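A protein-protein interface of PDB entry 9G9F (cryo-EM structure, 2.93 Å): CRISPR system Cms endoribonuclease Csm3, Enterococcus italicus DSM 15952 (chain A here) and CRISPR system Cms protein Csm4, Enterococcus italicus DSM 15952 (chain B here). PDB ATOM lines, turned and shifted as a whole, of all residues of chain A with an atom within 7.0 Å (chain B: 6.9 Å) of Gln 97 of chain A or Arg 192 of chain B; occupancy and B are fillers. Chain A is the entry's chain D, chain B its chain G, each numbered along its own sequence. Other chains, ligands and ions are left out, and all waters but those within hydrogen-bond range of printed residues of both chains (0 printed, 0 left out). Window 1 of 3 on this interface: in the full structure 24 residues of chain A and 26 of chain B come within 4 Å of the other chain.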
ATOM      1  N   TYR A   2       7.444  -9.166  -0.552  1.00  0.00           N
ATOM      2  CA  TYR A   2       8.569  -8.444   0.028  1.00  0.00           C
ATOM      3  C   TYR A   2       8.345  -8.205   1.505  1.00  0.00           C
ATOM      4  O   TYR A   2       7.214  -7.994   1.943  1.00  0.00           O
ATOM      5  CB  TYR A   2       8.779  -7.112  -0.681  1.00  0.00           C
ATOM      6  CG  TYR A   2      10.202  -6.613  -0.661  1.00  0.00           C
ATOM      7  CD1 TYR A   2      11.109  -7.022  -1.624  1.00  0.00           C
ATOM      8  CD2 TYR A   2      10.632  -5.722   0.306  1.00  0.00           C
ATOM      9  CE1 TYR A   2      12.405  -6.564  -1.621  1.00  0.00           C
ATOM     10  CE2 TYR A   2      11.928  -5.257   0.316  1.00  0.00           C
ATOM     11  CZ  TYR A   2      12.810  -5.682  -0.651  1.00  0.00           C
ATOM     12  OH  TYR A   2      14.106  -5.224  -0.652  1.00  0.00           O
ATOM     13  N   LYS A   4      10.259  -6.393   5.241  1.00  0.00           N
ATOM     14  CA  LYS A   4      11.264  -5.572   5.891  1.00  0.00           C
ATOM     15  C   LYS A   4      11.130  -5.769   7.388  1.00  0.00           C
ATOM     16  O   LYS A   4      10.038  -5.606   7.944  1.00  0.00           O
ATOM     17  CB  LYS A   4      11.111  -4.093   5.534  1.00  0.00           C
ATOM     18  CG  LYS A   4      11.583  -3.741   4.145  1.00  0.00           C
ATOM     19  CD  LYS A   4      11.083  -2.376   3.737  1.00  0.00           C
ATOM     20  CE  LYS A   4      11.538  -2.043   2.340  1.00  0.00           C
ATOM     21  NZ  LYS A   4      10.640  -1.051   1.725  1.00  0.00           N
ATOM     22  N   GLY A  48      24.957   6.245  10.530  1.00  0.00           N
ATOM     23  CA  GLY A  48      24.671   4.882  10.119  1.00  0.00           C
ATOM     24  C   GLY A  48      25.669   4.338   9.126  1.00  0.00           C
ATOM     25  O   GLY A  48      25.816   3.117   9.006  1.00  0.00           O
ATOM     26  N   LYS A  52      27.440   0.682   9.265  1.00  0.00           N
ATOM     27  CA  LYS A  52      27.408  -0.182   8.091  1.00  0.00           C
ATOM     28  C   LYS A  52      28.814  -0.541   7.636  1.00  0.00           C
ATOM     29  O   LYS A  52      29.090  -1.697   7.301  1.00  0.00           O
ATOM     30  CB  LYS A  52      26.628   0.493   6.966  1.00  0.00           C
ATOM     31  CG  LYS A  52      26.068  -0.466   5.938  1.00  0.00           C
ATOM     32  CD  LYS A  52      25.383   0.272   4.808  1.00  0.00           C
ATOM     33  CE  LYS A  52      24.851  -0.699   3.779  1.00  0.00           C
ATOM     34  NZ  LYS A  52      24.486  -0.035   2.506  1.00  0.00           N
ATOM     35  N   LEU A  82      24.332  -8.403   1.469  1.00  0.00           N
ATOM     36  CA  LEU A  82      23.858  -7.696   2.653  1.00  0.00           C
ATOM     37  C   LEU A  82      24.033  -6.189   2.514  1.00  0.00           C
ATOM     38  O   LEU A  82      23.112  -5.421   2.810  1.00  0.00           O
ATOM     39  CB  LEU A  82      24.589  -8.194   3.899  1.00  0.00           C
ATOM     40  CG  LEU A  82      23.927  -9.303   4.707  1.00  0.00           C
ATOM     41  CD1 LEU A  82      24.736  -9.562   5.958  1.00  0.00           C
ATOM     42  CD2 LEU A  82      22.501  -8.927   5.052  1.00  0.00           C
ATOM     43  N   SER A  93      20.672  -4.770  -4.501  1.00  0.00           N
ATOM     44  CA  SER A  93      20.229  -3.763  -3.549  1.00  0.00           C
ATOM     45  C   SER A  93      20.655  -4.164  -2.145  1.00  0.00           C
ATOM     46  O   SER A  93      20.480  -5.316  -1.739  1.00  0.00           O
ATOM     47  CB  SER A  93      18.713  -3.599  -3.619  1.00  0.00           C
ATOM     48  OG  SER A  93      18.292  -3.336  -4.945  1.00  0.00           O
ATOM     49  N   SER A  94      21.223  -3.215  -1.406  1.00  0.00           N
ATOM     50  CA  SER A  94      21.643  -3.492  -0.042  1.00  0.00           C
ATOM     51  C   SER A  94      20.439  -3.834   0.822  1.00  0.00           C
ATOM     52  O   SER A  94      19.396  -3.180   0.750  1.00  0.00           O
ATOM     53  CB  SER A  94      22.385  -2.293   0.541  1.00  0.00           C
ATOM     54  OG  SER A  94      22.791  -2.549   1.871  1.00  0.00           O
ATOM     55  N   ARG A  95      20.586  -4.876   1.637  1.00  0.00           N
ATOM     56  CA  ARG A  95      19.504  -5.333   2.498  1.00  0.00           C
ATOM     57  C   ARG A  95      19.523  -4.677   3.869  1.00  0.00           C
ATOM     58  O   ARG A  95      18.477  -4.582   4.515  1.00  0.00           O
ATOM     59  CB  ARG A  95      19.566  -6.851   2.660  1.00  0.00           C
ATOM     60  CG  ARG A  95      19.447  -7.613   1.362  1.00  0.00           C
ATOM     61  CD  ARG A  95      19.354  -9.099   1.618  1.00  0.00           C
ATOM     62  NE  ARG A  95      19.587  -9.880   0.411  1.00  0.00           N
ATOM     63  CZ  ARG A  95      19.325 -11.173   0.300  1.00  0.00           C
ATOM     64  NH1 ARG A  95      18.794 -11.858   1.299  1.00  0.00           N
ATOM     65  NH2 ARG A  95      19.601 -11.796  -0.841  1.00  0.00           N
ATOM     66  N   LEU A  96      20.683  -4.228   4.333  1.00  0.00           N
ATOM     67  CA  LEU A  96      20.791  -3.582   5.632  1.00  0.00           C
ATOM     68  C   LEU A  96      20.774  -2.072   5.453  1.00  0.00           C
ATOM     69  O   LEU A  96      21.720  -1.495   4.911  1.00  0.00           O
ATOM     70  CB  LEU A  96      22.063  -4.017   6.354  1.00  0.00           C
ATOM     71  CG  LEU A  96      22.032  -5.388   7.017  1.00  0.00           C
ATOM     72  CD1 LEU A  96      23.118  -5.471   8.060  1.00  0.00           C
ATOM     73  CD2 LEU A  96      20.680  -5.646   7.638  1.00  0.00           C
ATOM     74  N   GLN A  97      19.704  -1.439   5.907  1.00  0.00           N
ATOM     75  CA  GLN A  97      19.604   0.014   5.966  1.00  0.00           C
ATOM     76  C   GLN A  97      19.779   0.402   7.426  1.00  0.00           C
ATOM     77  O   GLN A  97      18.854   0.260   8.230  1.00  0.00           O
ATOM     78  CB  GLN A  97      18.271   0.492   5.407  1.00  0.00           C
ATOM     79  CG  GLN A  97      17.851  -0.234   4.158  1.00  0.00           C
ATOM     80  CD  GLN A  97      16.723   0.459   3.449  1.00  0.00           C
ATOM     81  OE1 GLN A  97      15.577   0.025   3.512  1.00  0.00           O
ATOM     82  NE2 GLN A  97      17.040   1.547   2.763  1.00  0.00           N
ATOM     83  N   ILE A  98      20.972   0.866   7.772  1.00  0.00           N
ATOM     84  CA  ILE A  98      21.333   1.159   9.152  1.00  0.00           C
ATOM     85  C   ILE A  98      21.226   2.667   9.333  1.00  0.00           C
ATOM     86  O   ILE A  98      22.113   3.417   8.923  1.00  0.00           O
ATOM     87  CB  ILE A  98      22.731   0.640   9.486  1.00  0.00           C
ATOM     88  CG1 ILE A  98      22.827  -0.846   9.147  1.00  0.00           C
ATOM     89  CG2 ILE A  98      23.053   0.880  10.950  1.00  0.00           C
ATOM     90  CD1 ILE A  98      24.193  -1.428   9.359  1.00  0.00           C
ATOM     91  N   SER A  99      20.140   3.114   9.959  1.00  0.00           N
ATOM     92  CA  SER A  99      19.926   4.538  10.146  1.00  0.00           C
ATOM     93  C   SER A  99      20.882   5.087  11.200  1.00  0.00           C
ATOM     94  O   SER A  99      21.494   4.344  11.968  1.00  0.00           O
ATOM     95  CB  SER A  99      18.481   4.810  10.558  1.00  0.00           C
ATOM     96  OG  SER A  99      17.580   4.088   9.737  1.00  0.00           O
ATOM     97  N   HIS A 151      18.986   1.915  14.814  1.00  0.00           N
ATOM     98  CA  HIS A 151      17.839   1.477  14.032  1.00  0.00           C
ATOM     99  C   HIS A 151      18.350   0.785  12.778  1.00  0.00           C
ATOM    100  O   HIS A 151      19.186   1.343  12.064  1.00  0.00           O
ATOM    101  CB  HIS A 151      16.952   2.675  13.676  1.00  0.00           C
ATOM    102  CG  HIS A 151      15.636   2.307  13.073  1.00  0.00           C
ATOM    103  ND1 HIS A 151      14.685   1.577  13.753  1.00  0.00           N
ATOM    104  CD2 HIS A 151      15.118   2.548  11.847  1.00  0.00           C
ATOM    105  CE1 HIS A 151      13.635   1.394  12.974  1.00  0.00           C
ATOM    106  NE2 HIS A 151      13.872   1.974  11.812  1.00  0.00           N
ATOM    107  N   ILE A 152      17.858  -0.424  12.515  1.00  0.00           N
ATOM    108  CA  ILE A 152      18.279  -1.203  11.358  1.00  0.00           C
ATOM    109  C   ILE A 152      17.040  -1.745  10.663  1.00  0.00           C
ATOM    110  O   ILE A 152      16.068  -2.130  11.321  1.00  0.00           O
ATOM    111  CB  ILE A 152      19.226  -2.352  11.763  1.00  0.00           C
ATOM    112  CG1 ILE A 152      20.573  -1.801  12.225  1.00  0.00           C
ATOM    113  CG2 ILE A 152      19.426  -3.326  10.619  1.00  0.00           C
ATOM    114  CD1 ILE A 152      21.590  -2.872  12.539  1.00  0.00           C
ATOM    115  N   ILE A 153      17.060  -1.752   9.335  1.00  0.00           N
ATOM    116  CA  ILE A 153      16.021  -2.381   8.531  1.00  0.00           C
ATOM    117  C   ILE A 153      16.678  -3.453   7.674  1.00  0.00           C
ATOM    118  O   ILE A 153      17.711  -3.201   7.044  1.00  0.00           O
ATOM    119  CB  ILE A 153      15.274  -1.359   7.656  1.00  0.00           C
ATOM    120  CG1 ILE A 153      14.537  -0.345   8.527  1.00  0.00           C
ATOM    121  CG2 ILE A 153      14.293  -2.060   6.738  1.00  0.00           C
ATOM    122  CD1 ILE A 153      13.229  -0.849   9.078  1.00  0.00           C
ATOM    123  N   TYR A 154      16.100  -4.648   7.671  1.00  0.00           N
ATOM    124  CA  TYR A 154      16.555  -5.737   6.821  1.00  0.00           C
ATOM    125  C   TYR A 154      15.539  -5.955   5.710  1.00  0.00           C
ATOM    126  O   TYR A 154      14.338  -6.059   5.979  1.00  0.00           O
ATOM    127  CB  TYR A 154      16.749  -7.026   7.619  1.00  0.00           C
ATOM    128  CG  TYR A 154      17.185  -8.196   6.769  1.00  0.00           C
ATOM    129  CD1 TYR A 154      18.526  -8.408   6.487  1.00  0.00           C
ATOM    130  CD2 TYR A 154      16.256  -9.083   6.244  1.00  0.00           C
ATOM    131  CE1 TYR A 154      18.928  -9.469   5.709  1.00  0.00           C
ATOM    132  CE2 TYR A 154      16.649 -10.146   5.466  1.00  0.00           C
ATOM    133  CZ  TYR A 154      17.986 -10.336   5.202  1.00  0.00           C
ATOM    134  OH  TYR A 154      18.382 -11.397   4.424  1.00  0.00           O
ATOM    135  N   ASN A 155      16.025  -6.019   4.470  1.00  0.00           N
ATOM    136  CA  ASN A 155      15.190  -6.232   3.294  1.00  0.00           C
ATOM    137  C   ASN A 155      15.213  -7.713   2.939  1.00  0.00           C
ATOM    138  O   ASN A 155      16.242  -8.239   2.509  1.00  0.00           O
ATOM    139  CB  ASN A 155      15.682  -5.397   2.116  1.00  0.00           C
ATOM    140  CG  ASN A 155      15.615  -3.915   2.382  1.00  0.00           C
ATOM    141  OD1 ASN A 155      16.594  -3.303   2.801  1.00  0.00           O
ATOM    142  ND2 ASN A 155      14.448  -3.331   2.166  1.00  0.00           N
ATOM    143  N   HIS B  18      19.245  13.299   2.200  1.00  0.00           N
ATOM    144  CA  HIS B  18      20.191  13.842   1.232  1.00  0.00           C
ATOM    145  C   HIS B  18      19.499  14.789   0.260  1.00  0.00           C
ATOM    146  O   HIS B  18      19.810  15.985   0.215  1.00  0.00           O
ATOM    147  CB  HIS B  18      20.890  12.721   0.472  1.00  0.00           C
ATOM    148  CG  HIS B  18      21.906  13.215  -0.506  1.00  0.00           C
ATOM    149  ND1 HIS B  18      21.769  13.060  -1.866  1.00  0.00           N
ATOM    150  CD2 HIS B  18      23.069  13.879  -0.320  1.00  0.00           C
ATOM    151  CE1 HIS B  18      22.807  13.602  -2.474  1.00  0.00           C
ATOM    152  NE2 HIS B  18      23.612  14.103  -1.559  1.00  0.00           N
ATOM    153  N   ILE B  42       9.297   2.209  -7.718  1.00  0.00           N
ATOM    154  CA  ILE B  42      10.220   1.225  -7.161  1.00  0.00           C
ATOM    155  C   ILE B  42       9.543   0.437  -6.051  1.00  0.00           C
ATOM    156  O   ILE B  42       9.663  -0.793  -5.977  1.00  0.00           O
ATOM    157  CB  ILE B  42      11.502   1.910  -6.657  1.00  0.00           C
ATOM    158  CG1 ILE B  42      12.352   2.390  -7.828  1.00  0.00           C
ATOM    159  CG2 ILE B  42      12.299   0.967  -5.780  1.00  0.00           C
ATOM    160  CD1 ILE B  42      13.657   2.995  -7.408  1.00  0.00           C
ATOM    161  N   GLU B  43       8.809   1.127  -5.178  1.00  0.00           N
ATOM    162  CA  GLU B  43       8.120   0.440  -4.091  1.00  0.00           C
ATOM    163  C   GLU B  43       7.068  -0.523  -4.621  1.00  0.00           C
ATOM    164  O   GLU B  43       6.973  -1.665  -4.161  1.00  0.00           O
ATOM    165  CB  GLU B  43       7.488   1.459  -3.147  1.00  0.00           C
ATOM    166  CG  GLU B  43       7.482   1.013  -1.709  1.00  0.00           C
ATOM    167  CD  GLU B  43       8.880   0.809  -1.176  1.00  0.00           C
ATOM    168  OE1 GLU B  43       9.806   1.515  -1.628  1.00  0.00           O
ATOM    169  OE2 GLU B  43       9.054  -0.068  -0.308  1.00  0.00           O
ATOM    170  N   GLN B  46       8.773  -3.580  -5.828  1.00  0.00           N
ATOM    171  CA  GLN B  46       9.255  -4.432  -4.746  1.00  0.00           C
ATOM    172  C   GLN B  46       8.104  -5.144  -4.048  1.00  0.00           C
ATOM    173  O   GLN B  46       8.189  -6.343  -3.761  1.00  0.00           O
ATOM    174  CB  GLN B  46      10.066  -3.610  -3.748  1.00  0.00           C
ATOM    175  CG  GLN B  46      11.443  -3.230  -4.250  1.00  0.00           C
ATOM    176  CD  GLN B  46      12.232  -2.423  -3.242  1.00  0.00           C
ATOM    177  OE1 GLN B  46      11.839  -2.300  -2.084  1.00  0.00           O
ATOM    178  NE2 GLN B  46      13.353  -1.866  -3.678  1.00  0.00           N
ATOM    179  N   LEU B 183       7.373   2.855   2.189  1.00  0.00           N
ATOM    180  CA  LEU B 183       8.409   3.860   1.975  1.00  0.00           C
ATOM    181  C   LEU B 183       8.929   4.429   3.283  1.00  0.00           C
ATOM    182  O   LEU B 183      10.069   4.903   3.333  1.00  0.00           O
ATOM    183  CB  LEU B 183       7.865   4.988   1.099  1.00  0.00           C
ATOM    184  CG  LEU B 183       8.326   5.084  -0.351  1.00  0.00           C
ATOM    185  CD1 LEU B 183       7.695   6.284  -1.010  1.00  0.00           C
ATOM    186  CD2 LEU B 183       9.827   5.202  -0.400  1.00  0.00           C
ATOM    187  N   TYR B 185      10.029   2.973   5.728  1.00  0.00           N
ATOM    188  CA  TYR B 185      11.221   2.211   6.067  1.00  0.00           C
ATOM    189  C   TYR B 185      12.148   1.996   4.882  1.00  0.00           C
ATOM    190  O   TYR B 185      13.342   1.759   5.084  1.00  0.00           O
ATOM    191  CB  TYR B 185      10.820   0.858   6.656  1.00  0.00           C
ATOM    192  CG  TYR B 185       9.604   0.947   7.544  1.00  0.00           C
ATOM    193  CD1 TYR B 185       9.716   1.341   8.867  1.00  0.00           C
ATOM    194  CD2 TYR B 185       8.342   0.655   7.050  1.00  0.00           C
ATOM    195  CE1 TYR B 185       8.605   1.431   9.676  1.00  0.00           C
ATOM    196  CE2 TYR B 185       7.227   0.742   7.850  1.00  0.00           C
ATOM    197  CZ  TYR B 185       7.363   1.130   9.162  1.00  0.00           C
ATOM    198  OH  TYR B 185       6.246   1.214   9.959  1.00  0.00           O
ATOM    199  N   SER B 186      11.633   2.065   3.651  1.00  0.00           N
ATOM    200  CA  SER B 186      12.523   2.025   2.494  1.00  0.00           C
ATOM    201  C   SER B 186      13.434   3.243   2.460  1.00  0.00           C
ATOM    202  O   SER B 186      14.617   3.133   2.124  1.00  0.00           O
ATOM    203  CB  SER B 186      11.719   1.935   1.202  1.00  0.00           C
ATOM    204  OG  SER B 186      12.582   1.930   0.080  1.00  0.00           O
ATOM    205  N   GLY B 187      12.905   4.404   2.799  1.00  0.00           N
ATOM    206  CA  GLY B 187      13.671   5.631   2.753  1.00  0.00           C
ATOM    207  C   GLY B 187      13.426   6.399   1.470  1.00  0.00           C
ATOM    208  O   GLY B 187      13.013   5.844   0.446  1.00  0.00           O
ATOM    209  N   ILE B 188      13.672   7.704   1.522  1.00  0.00           N
ATOM    210  CA  ILE B 188      13.509   8.566   0.361  1.00  0.00           C
ATOM    211  C   ILE B 188      14.739   9.453   0.240  1.00  0.00           C
ATOM    212  O   ILE B 188      15.446   9.710   1.218  1.00  0.00           O
ATOM    213  CB  ILE B 188      12.215   9.402   0.448  1.00  0.00           C
ATOM    214  CG1 ILE B 188      11.662   9.678  -0.946  1.00  0.00           C
ATOM    215  CG2 ILE B 188      12.457  10.698   1.174  1.00  0.00           C
ATOM    216  CD1 ILE B 188      10.221  10.097  -0.940  1.00  0.00           C
ATOM    217  N   GLY B 189      15.006   9.906  -0.978  1.00  0.00           N
ATOM    218  CA  GLY B 189      16.208  10.653  -1.265  1.00  0.00           C
ATOM    219  C   GLY B 189      17.412   9.753  -1.459  1.00  0.00           C
ATOM    220  O   GLY B 189      17.350   8.530  -1.332  1.00  0.00           O
ATOM    221  N   GLY B 190      18.534  10.380  -1.784  1.00  0.00           N
ATOM    222  CA  GLY B 190      19.758   9.637  -1.974  1.00  0.00           C
ATOM    223  C   GLY B 190      20.346   9.162  -0.664  1.00  0.00           C
ATOM    224  O   GLY B 190      19.981   9.619   0.416  1.00  0.00           O
ATOM    225  N   LYS B 191      21.274   8.214  -0.773  1.00  0.00           N
ATOM    226  CA  LYS B 191      21.934   7.613   0.387  1.00  0.00           C
ATOM    227  C   LYS B 191      20.923   7.044   1.375  1.00  0.00           C
ATOM    228  O   LYS B 191      21.145   7.055   2.584  1.00  0.00           O
ATOM    229  CB  LYS B 191      22.859   8.612   1.081  1.00  0.00           C
ATOM    230  CG  LYS B 191      24.329   8.269   0.985  1.00  0.00           C
ATOM    231  CD  LYS B 191      24.734   7.988  -0.445  1.00  0.00           C
ATOM    232  CE  LYS B 191      26.240   7.885  -0.585  1.00  0.00           C
ATOM    233  NZ  LYS B 191      26.808   6.781   0.225  1.00  0.00           N
ATOM    234  N   ARG B 192      19.804   6.531   0.864  1.00  0.00           N
ATOM    235  CA  ARG B 192      18.779   5.964   1.728  1.00  0.00           C
ATOM    236  C   ARG B 192      19.200   4.641   2.345  1.00  0.00           C
ATOM    237  O   ARG B 192      18.525   4.165   3.262  1.00  0.00           O
ATOM    238  CB  ARG B 192      17.481   5.781   0.948  1.00  0.00           C
ATOM    239  CG  ARG B 192      17.619   4.888  -0.262  1.00  0.00           C
ATOM    240  CD  ARG B 192      16.318   4.772  -1.020  1.00  0.00           C
ATOM    241  NE  ARG B 192      16.459   3.915  -2.189  1.00  0.00           N
ATOM    242  CZ  ARG B 192      16.314   2.598  -2.176  1.00  0.00           C
ATOM    243  NH1 ARG B 192      16.014   1.949  -1.065  1.00  0.00           N
ATOM    244  NH2 ARG B 192      16.472   1.916  -3.304  1.00  0.00           N
ATOM    245  N   SER B 193      20.280   4.031   1.861  1.00  0.00           N
ATOM    246  CA  SER B 193      20.807   2.804   2.437  1.00  0.00           C
ATOM    247  C   SER B 193      21.969   3.045   3.387  1.00  0.00           C
ATOM    248  O   SER B 193      22.438   2.094   4.016  1.00  0.00           O
ATOM    249  CB  SER B 193      21.256   1.848   1.328  1.00  0.00           C
ATOM    250  OG  SER B 193      20.204   1.595   0.415  1.00  0.00           O
ATOM    251  N   ALA B 194      22.446   4.283   3.502  1.00  0.00           N
ATOM    252  CA  ALA B 194      23.564   4.615   4.376  1.00  0.00           C
ATOM    253  C   ALA B 194      23.146   5.506   5.541  1.00  0.00           C
ATOM    254  O   ALA B 194      23.988   6.206   6.112  1.00  0.00           O
ATOM    255  CB  ALA B 194      24.688   5.274   3.578  1.00  0.00           C
ATOM    256  N   GLY B 195      21.864   5.510   5.897  1.00  0.00           N
ATOM    257  CA  GLY B 195      21.389   6.150   7.109  1.00  0.00           C
ATOM    258  C   GLY B 195      20.469   7.331   6.899  1.00  0.00           C
ATOM    259  O   GLY B 195      19.923   7.854   7.880  1.00  0.00           O
ATOM    260  N   TYR B 196      20.281   7.782   5.667  1.00  0.00           N
ATOM    261  CA  TYR B 196      19.461   8.954   5.411  1.00  0.00           C
ATOM    262  C   TYR B 196      18.079   8.561   4.902  1.00  0.00           C
ATOM    263  O   TYR B 196      17.833   7.428   4.493  1.00  0.00           O
ATOM    264  CB  TYR B 196      20.154   9.871   4.410  1.00  0.00           C
ATOM    265  CG  TYR B 196      21.463  10.409   4.916  1.00  0.00           C
ATOM    266  CD1 TYR B 196      21.628  10.726   6.247  1.00  0.00           C
ATOM    267  CD2 TYR B 196      22.535  10.597   4.066  1.00  0.00           C
ATOM    268  CE1 TYR B 196      22.814  11.218   6.717  1.00  0.00           C
ATOM    269  CE2 TYR B 196      23.727  11.087   4.530  1.00  0.00           C
ATOM    270  CZ  TYR B 196      23.859  11.395   5.856  1.00  0.00           C
ATOM    271  OH  TYR B 196      25.044  11.888   6.335  1.00  0.00           O
ATOM    272  N   GLY B 197      17.164   9.519   4.948  1.00  0.00           N
ATOM    273  CA  GLY B 197      15.893   9.386   4.277  1.00  0.00           C
ATOM    274  C   GLY B 197      14.811   8.660   5.037  1.00  0.00           C
ATOM    275  O   GLY B 197      13.694   8.546   4.522  1.00  0.00           O
ATOM    276  N   GLN B 198      15.093   8.159   6.233  1.00  0.00           N
ATOM    277  CA  GLN B 198      14.062   7.483   7.005  1.00  0.00           C
ATOM    278  C   GLN B 198      13.020   8.492   7.470  1.00  0.00           C
ATOM    279  O   GLN B 198      13.358   9.572   7.955  1.00  0.00           O
ATOM    280  CB  GLN B 198      14.685   6.771   8.205  1.00  0.00           C
ATOM    281  CG  GLN B 198      14.152   5.377   8.444  1.00  0.00           C
ATOM    282  CD  GLN B 198      14.638   4.385   7.412  1.00  0.00           C
ATOM    283  OE1 GLN B 198      13.966   3.401   7.124  1.00  0.00           O
ATOM    284  NE2 GLN B 198      15.816   4.633   6.856  1.00  0.00           N
ATOM    285  N   GLN B 252      18.271   3.758 -11.332  1.00  0.00           N
ATOM    286  CA  GLN B 252      18.379   2.962 -10.111  1.00  0.00           C
ATOM    287  C   GLN B 252      17.506   1.723 -10.273  1.00  0.00           C
ATOM    288  O   GLN B 252      16.292   1.774 -10.054  1.00  0.00           O
ATOM    289  CB  GLN B 252      17.964   3.776  -8.891  1.00  0.00           C
ATOM    290  CG  GLN B 252      17.926   2.983  -7.604  1.00  0.00           C
ATOM    291  CD  GLN B 252      17.437   3.805  -6.437  1.00  0.00           C
ATOM    292  OE1 GLN B 252      16.403   3.506  -5.847  1.00  0.00           O
ATOM    293  NE2 GLN B 252      18.180   4.844  -6.093  1.00  0.00           N
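NZ of Lys 4 of chain A is in salt-bridge range of OE2 of Glu 43 of chain B, 2.8 Å away. The side-chain amino group of Lys 52 of chain A lies within hydrogen-bond range of the backbone carbonyl oxygen of Ser 193 of chain B, 3.3 Å away. OE1 of Gln 97 of chain A lies close to O of Tyr 185 of chain B (3.2 Å). NE2 of Gln 97 of chain A lies within hydrogen-bond range of O of Ser 186 of chain B (3.0 Å). The backbone carbonyl oxygen (O) of Arg 192 of chain B sits at hydrogen-bond distance from the side-chain amide nitrogen (NE2) of Gln 97 of chain A (3.1 Å). The side-chain amide nitrogen (NE2) of Gln 198 of chain B is in hydrogen-bond range of the side-chain hydroxyl (OG) of Ser 99 of chain A, at 3.4 Å.
NZ of Lys 52 of chain A sits at hydrogen-bond distance from OG of Ser 94 of chain A (3.1 Å). The backbone carbonyl oxygen of Leu 82 of chain A lies within hydrogen-bond range of the backbone NH of Leu 96 of chain A. The backbone carbonyl oxygen (O) of Leu 96 of chain A is in hydrogen-bond range of the side-chain hydroxyl (OG) of Ser 94 of chain A. The backbone NH (N) of Ser 99 of chain A is in hydrogen-bond range of the backbone carbonyl oxygen (O) of His 151 of chain A, at 2.9 Å. O of Tyr 185 of chain B lies close to OE1 of Gln 198 of chain B (2.7 Å). The guanidinium group (NH2) of Arg 192 of chain B is in hydrogen-bond range of the side-chain amide oxygen (OE1) of Gln 252 of chain B.
Among the printed residues, merely in contact across the chains: Lys 4 of chain A with Ser 186 of chain B (3.2 Å), Tyr 2 of chain A with Gln 46 of chain B (3.2 Å), Ile 98 of chain A with Gly 195 of chain B (3.4 Å), Ser 99 of chain A with Gly 195 of chain B (3.7 Å), Leu 96 of chain A with Ser 193 of chain B (3.8 Å), Ile 153 of chain A with Tyr 185 of chain B (3.8 Å), Gly 48 of chain A with Ala 194 of chain B (3.9 Å) and Gln 97 of chain A with Ser 193 of chain B (3.9 Å).
Gln 97 of chain A touches just these residues of chain B: Tyr 185, Ser 186, Arg 192 and Ser 193. Of chain A, only Gln 97 comes within 4 Å of Arg 192 of chain B. Printed residues of chain A within 4 Å of Gly 195 of chain B: Ile 98 (3.4 Å) and Ser 99 (3.7 Å). Of the printed residues of chain A, Ser 186 of chain B touches Lys 4 (3.2 Å) and Gln 97 (3.0 Å). Of the printed residues of chain B, Ile 153 of chain A touches Tyr 185 (3.8 Å). Printed residues of chain B within 4 Å of Ser 99 of chain A: Gly 195 (3.7 Å) and Gln 198 (3.4 Å). Leu 82 of chain A touches none of the printed residues of chain B. Gly 189 of chain B touches none of the printed residues of chain A. The nearest residue of chain A that does not touch Arg 192 of chain B is Ser 93 of chain A (5.8 Å). The nearest printed residue of chain B that does not touch Ser 99 of chain A is Tyr 196 of chain B (5.5 Å).
Printed residues of chain B that touch a printed residue of chain A: Glu 43, Gln 46, Tyr 185, Ser 186, Arg 192, Ser 193, Ala 194, Gly 195 and Gln 198. Hydrophobic or aromatic side chains of chain B within 4 Å of the printed part of chain A: Tyr 185. Along chain A the printed residues that touch a printed residue of chain B span positions 2 to 153.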
